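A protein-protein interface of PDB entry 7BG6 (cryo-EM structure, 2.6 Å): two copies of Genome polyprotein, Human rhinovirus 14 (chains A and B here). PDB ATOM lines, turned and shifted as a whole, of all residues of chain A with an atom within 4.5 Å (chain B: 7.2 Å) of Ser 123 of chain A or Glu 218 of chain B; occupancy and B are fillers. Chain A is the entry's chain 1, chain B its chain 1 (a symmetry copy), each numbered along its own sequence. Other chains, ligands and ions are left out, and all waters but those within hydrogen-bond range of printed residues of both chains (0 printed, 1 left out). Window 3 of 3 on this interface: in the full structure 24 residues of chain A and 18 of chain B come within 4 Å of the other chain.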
ATOM      1  N   GLN A 120     -22.828 -10.629   9.908  1.00  0.00           N
ATOM      2  CA  GLN A 120     -22.316  -9.269   9.856  1.00  0.00           C
ATOM      3  C   GLN A 120     -20.809  -9.315  10.102  1.00  0.00           C
ATOM      4  O   GLN A 120     -20.360  -9.134  11.232  1.00  0.00           O
ATOM      5  CB  GLN A 120     -23.030  -8.378  10.875  1.00  0.00           C
ATOM      6  CG  GLN A 120     -24.532  -8.245  10.654  1.00  0.00           C
ATOM      7  CD  GLN A 120     -25.346  -9.337  11.307  1.00  0.00           C
ATOM      8  OE1 GLN A 120     -24.844 -10.130  12.100  1.00  0.00           O
ATOM      9  NE2 GLN A 120     -26.626  -9.384  10.974  1.00  0.00           N
ATOM     10  N   PRO A 121     -19.984  -9.565   9.055  1.00  0.00           N
ATOM     11  CA  PRO A 121     -18.541  -9.750   9.231  1.00  0.00           C
ATOM     12  C   PRO A 121     -17.832  -8.504   9.755  1.00  0.00           C
ATOM     13  O   PRO A 121     -16.797  -8.608  10.412  1.00  0.00           O
ATOM     14  CB  PRO A 121     -18.037 -10.107   7.823  1.00  0.00           C
ATOM     15  CG  PRO A 121     -19.087  -9.543   6.889  1.00  0.00           C
ATOM     16  CD  PRO A 121     -20.393  -9.670   7.645  1.00  0.00           C
ATOM     17  N   ASP A 122     -18.402  -7.331   9.453  1.00  0.00           N
ATOM     18  CA  ASP A 122     -17.875  -6.060   9.919  1.00  0.00           C
ATOM     19  C   ASP A 122     -18.655  -5.612  11.154  1.00  0.00           C
ATOM     20  O   ASP A 122     -19.622  -6.261  11.551  1.00  0.00           O
ATOM     21  CB  ASP A 122     -17.878  -5.013   8.801  1.00  0.00           C
ATOM     22  CG  ASP A 122     -17.019  -5.389   7.604  1.00  0.00           C
ATOM     23  OD1 ASP A 122     -15.996  -6.077   7.805  1.00  0.00           O
ATOM     24  OD2 ASP A 122     -17.381  -4.993   6.479  1.00  0.00           O
ATOM     25  N   SER A 123     -18.216  -4.493  11.744  1.00  0.00           N
ATOM     26  CA  SER A 123     -18.794  -3.947  12.962  1.00  0.00           C
ATOM     27  C   SER A 123     -20.306  -3.795  12.814  1.00  0.00           C
ATOM     28  O   SER A 123     -20.783  -3.129  11.897  1.00  0.00           O
ATOM     29  CB  SER A 123     -18.141  -2.639  13.333  1.00  0.00           C
ATOM     30  OG  SER A 123     -18.356  -1.662  12.325  1.00  0.00           O
ATOM     31  N   ALA A 124     -21.042  -4.442  13.725  1.00  0.00           N
ATOM     32  CA  ALA A 124     -22.490  -4.342  13.797  1.00  0.00           C
ATOM     33  C   ALA A 124     -22.920  -4.390  15.258  1.00  0.00           C
ATOM     34  O   ALA A 124     -22.340  -5.126  16.053  1.00  0.00           O
ATOM     35  CB  ALA A 124     -23.129  -5.449  12.997  1.00  0.00           C
ATOM     36  N   HIS A 219     -24.883  -0.942   8.943  1.00  0.00           N
ATOM     37  CA  HIS A 219     -23.949  -2.048   8.820  1.00  0.00           C
ATOM     38  C   HIS A 219     -24.379  -2.974   7.686  1.00  0.00           C
ATOM     39  O   HIS A 219     -25.569  -3.112   7.408  1.00  0.00           O
ATOM     40  CB  HIS A 219     -23.825  -2.797  10.156  1.00  0.00           C
ATOM     41  CG  HIS A 219     -25.106  -3.395  10.631  1.00  0.00           C
ATOM     42  ND1 HIS A 219     -25.569  -4.614  10.171  1.00  0.00           N
ATOM     43  CD2 HIS A 219     -26.024  -2.953  11.518  1.00  0.00           C
ATOM     44  CE1 HIS A 219     -26.716  -4.895  10.755  1.00  0.00           C
ATOM     45  NE2 HIS A 219     -27.016  -3.892  11.587  1.00  0.00           N
ATOM     46  N   SER B 123     -15.664  -9.677  23.528  1.00  0.00           N
ATOM     47  CA  SER B 123     -16.495  -8.541  23.164  1.00  0.00           C
ATOM     48  C   SER B 123     -17.402  -8.897  21.989  1.00  0.00           C
ATOM     49  O   SER B 123     -16.929  -9.310  20.933  1.00  0.00           O
ATOM     50  CB  SER B 123     -15.651  -7.328  22.862  1.00  0.00           C
ATOM     51  OG  SER B 123     -14.802  -7.567  21.748  1.00  0.00           O
ATOM     52  N   ALA B 124     -18.714  -8.745  22.208  1.00  0.00           N
ATOM     53  CA  ALA B 124     -19.721  -8.949  21.181  1.00  0.00           C
ATOM     54  C   ALA B 124     -20.852  -7.948  21.388  1.00  0.00           C
ATOM     55  O   ALA B 124     -21.218  -7.648  22.522  1.00  0.00           O
ATOM     56  CB  ALA B 124     -20.228 -10.369  21.224  1.00  0.00           C
ATOM     57  N   ASN B 125     -21.397  -7.444  20.275  1.00  0.00           N
ATOM     58  CA  ASN B 125     -22.417  -6.409  20.312  1.00  0.00           C
ATOM     59  C   ASN B 125     -23.805  -7.040  20.381  1.00  0.00           C
ATOM     60  O   ASN B 125     -24.745  -6.413  20.866  1.00  0.00           O
ATOM     61  CB  ASN B 125     -22.295  -5.447  19.127  1.00  0.00           C
ATOM     62  CG  ASN B 125     -21.001  -4.660  19.117  1.00  0.00           C
ATOM     63  OD1 ASN B 125     -20.627  -4.053  20.119  1.00  0.00           O
ATOM     64  ND2 ASN B 125     -20.316  -4.653  17.986  1.00  0.00           N
ATOM     65  N   TYR B 126     -23.919  -8.282  19.897  1.00  0.00           N
ATOM     66  CA  TYR B 126     -25.208  -8.942  19.763  1.00  0.00           C
ATOM     67  C   TYR B 126     -25.044 -10.457  19.857  1.00  0.00           C
ATOM     68  O   TYR B 126     -23.940 -10.981  19.722  1.00  0.00           O
ATOM     69  CB  TYR B 126     -25.873  -8.547  18.441  1.00  0.00           C
ATOM     70  CG  TYR B 126     -25.057  -8.851  17.209  1.00  0.00           C
ATOM     71  CD1 TYR B 126     -25.238 -10.030  16.503  1.00  0.00           C
ATOM     72  CD2 TYR B 126     -24.096  -7.961  16.750  1.00  0.00           C
ATOM     73  CE1 TYR B 126     -24.488 -10.320  15.374  1.00  0.00           C
ATOM     74  CE2 TYR B 126     -23.337  -8.236  15.624  1.00  0.00           C
ATOM     75  CZ  TYR B 126     -23.535  -9.418  14.933  1.00  0.00           C
ATOM     76  OH  TYR B 126     -22.791  -9.695  13.823  1.00  0.00           O
ATOM     77  N   SER B 128     -25.740 -13.631  17.935  1.00  0.00           N
ATOM     78  CA  SER B 128     -25.963 -14.039  16.557  1.00  0.00           C
ATOM     79  C   SER B 128     -27.045 -15.114  16.488  1.00  0.00           C
ATOM     80  O   SER B 128     -27.150 -15.956  17.378  1.00  0.00           O
ATOM     81  CB  SER B 128     -24.682 -14.510  15.919  1.00  0.00           C
ATOM     82  OG  SER B 128     -23.748 -13.447  15.812  1.00  0.00           O
ATOM     83  N   HIS B 216     -19.325 -16.106   9.131  1.00  0.00           N
ATOM     84  CA  HIS B 216     -18.725 -15.547  10.330  1.00  0.00           C
ATOM     85  C   HIS B 216     -19.264 -14.145  10.597  1.00  0.00           C
ATOM     86  O   HIS B 216     -19.664 -13.437   9.674  1.00  0.00           O
ATOM     87  CB  HIS B 216     -17.206 -15.477  10.147  1.00  0.00           C
ATOM     88  CG  HIS B 216     -16.806 -14.638   8.981  1.00  0.00           C
ATOM     89  ND1 HIS B 216     -16.869 -15.104   7.683  1.00  0.00           N
ATOM     90  CD2 HIS B 216     -16.370 -13.362   8.907  1.00  0.00           C
ATOM     91  CE1 HIS B 216     -16.475 -14.154   6.858  1.00  0.00           C
ATOM     92  NE2 HIS B 216     -16.165 -13.074   7.586  1.00  0.00           N
ATOM     93  N   ASP B 217     -19.255 -13.763  11.879  1.00  0.00           N
ATOM     94  CA  ASP B 217     -19.365 -12.373  12.286  1.00  0.00           C
ATOM     95  C   ASP B 217     -17.966 -11.888  12.659  1.00  0.00           C
ATOM     96  O   ASP B 217     -16.987 -12.597  12.432  1.00  0.00           O
ATOM     97  CB  ASP B 217     -20.389 -12.201  13.414  1.00  0.00           C
ATOM     98  CG  ASP B 217     -21.712 -12.901  13.147  1.00  0.00           C
ATOM     99  OD1 ASP B 217     -22.707 -12.195  12.887  1.00  0.00           O
ATOM    100  OD2 ASP B 217     -21.739 -14.147  13.210  1.00  0.00           O
ATOM    101  N   GLU B 218     -17.878 -10.680  13.228  1.00  0.00           N
ATOM    102  CA  GLU B 218     -16.599 -10.126  13.643  1.00  0.00           C
ATOM    103  C   GLU B 218     -16.183 -10.729  14.984  1.00  0.00           C
ATOM    104  O   GLU B 218     -14.995 -10.786  15.299  1.00  0.00           O
ATOM    105  CB  GLU B 218     -16.644  -8.595  13.688  1.00  0.00           C
ATOM    106  CG  GLU B 218     -17.529  -8.027  14.785  1.00  0.00           C
ATOM    107  CD  GLU B 218     -17.392  -6.532  15.026  1.00  0.00           C
ATOM    108  OE1 GLU B 218     -18.266  -5.967  15.712  1.00  0.00           O
ATOM    109  OE2 GLU B 218     -16.413  -5.936  14.531  1.00  0.00           O
ATOM    110  N   HIS B 219     -17.177 -11.179  15.759  1.00  0.00           N
ATOM    111  CA  HIS B 219     -16.955 -11.730  17.085  1.00  0.00           C
ATOM    112  C   HIS B 219     -17.049 -13.252  17.044  1.00  0.00           C
ATOM    113  O   HIS B 219     -17.792 -13.812  16.238  1.00  0.00           O
ATOM    114  CB  HIS B 219     -17.946 -11.123  18.091  1.00  0.00           C
ATOM    115  CG  HIS B 219     -19.375 -11.397  17.768  1.00  0.00           C
ATOM    116  ND1 HIS B 219     -19.998 -12.583  18.113  1.00  0.00           N
ATOM    117  CD2 HIS B 219     -20.308 -10.652  17.136  1.00  0.00           C
ATOM    118  CE1 HIS B 219     -21.251 -12.555  17.705  1.00  0.00           C
ATOM    119  NE2 HIS B 219     -21.466 -11.380  17.104  1.00  0.00           N
ATOM    120  N   LYS B 220     -16.291 -13.904  17.932  1.00  0.00           N
ATOM    121  CA  LYS B 220     -16.309 -15.350  18.063  1.00  0.00           C
ATOM    122  C   LYS B 220     -17.429 -15.753  19.017  1.00  0.00           C
ATOM    123  O   LYS B 220     -17.517 -15.241  20.133  1.00  0.00           O
ATOM    124  CB  LYS B 220     -14.949 -15.866  18.545  1.00  0.00           C
ATOM    125  CG  LYS B 220     -13.802 -15.703  17.557  1.00  0.00           C
ATOM    126  CD  LYS B 220     -12.472 -16.186  18.095  1.00  0.00           C
ATOM    127  CE  LYS B 220     -11.334 -15.989  17.117  1.00  0.00           C
ATOM    128  NZ  LYS B 220     -10.047 -16.480  17.665  1.00  0.00           N
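The backbone carbonyl oxygen of Ala 124 of chain A is in hydrogen-bond range of the side-chain amide nitrogen of Asn 125 of chain B, 2.8 Å away.
The side-chain amide oxygen (OE1) of Gln 120 of chain A lies close to the side-chain carboxylate (OD1) of Asp 217 of chain B (3.1 Å).
OE1 of Gln 120 of chain A is in hydrogen-bond range of OH of Tyr 126 of chain B (2.7 Å).
OD1 of Asp 217 of chain B sits at hydrogen-bond distance from OG of Ser 128 of chain B (3.3 Å).
OH of Tyr 126 of chain B is in hydrogen-bond range of OD1 of Asp 217 of chain B, 2.7 Å away.
The side-chain carboxylate (OE1) of Glu 218 of chain B lies within hydrogen-bond range of the side-chain amide nitrogen (ND2) of Asn 125 of chain B (3.3 Å).
Of the 6 printed residues of chain A, 4 touch a printed residue of chain B.
Of the 10 printed residues of chain B, 5 touch a printed residue of chain A.
Among the printed residues, 9 pairs touch across the chains.
Among the printed residues, no Asp or Glu carboxylate lies within 4 Å of a Lys or Arg side-chain nitrogen of the other chain.
Of chain B, only Glu 218 (3.5 Å) comes within 4 Å of Ser 123 of chain A.
Glu 218 of chain B touches just these residues of chain A: Gln 120 (3.5 Å), Pro 121 (3.3 Å), Ser 123 (3.5 Å) and Ala 124 (3.7 Å).
Printed residues of chain A within 4 Å of Asn 125 of chain B: Ala 124.
Printed residues of chain A within 4 Å of His 216 of chain B: Pro 121.
Printed residues of chain B within 4 Å of Pro 121 of chain A: His 216 and Glu 218.
Printed residues of chain A within 4 Å of Asp 217 of chain B: Gln 120 (3.1 Å).
Ala 124 of chain B touches none of the printed residues of chain A.
Lys 220 of chain B touches none of the printed residues of chain A.
The nearest residue of chain B that does not touch Ser 123 of chain A is Asn 125 of chain B (5.2 Å).
The nearest residue of chain A that does not touch Glu 218 of chain B is Asp 122 of chain A (4.1 Å).
The nearest printed residue of chain B that does not touch Pro 121 of chain A is Asp 217 of chain B (4.1 Å).
3 positions are printed for both chains.
Of the 9 pairs that touch across the chains among the printed residues, none has its exchanged pair printed and touching as well.
Among the printed residues, merely in contact across the chains: Pro 121 of chain A with Glu 218 of chain B (3.3 Å), Ala 124 of chain A with Tyr 126 of chain B (3.3 Å), Ser 123 of chain A with Glu 218 of chain B (3.5 Å), Pro 121 of chain A with His 216 of chain B (3.5 Å), Gln 120 of chain A with Glu 218 of chain B (3.5 Å) and Ala 124 of chain A with Glu 218 of chain B (3.7 Å).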
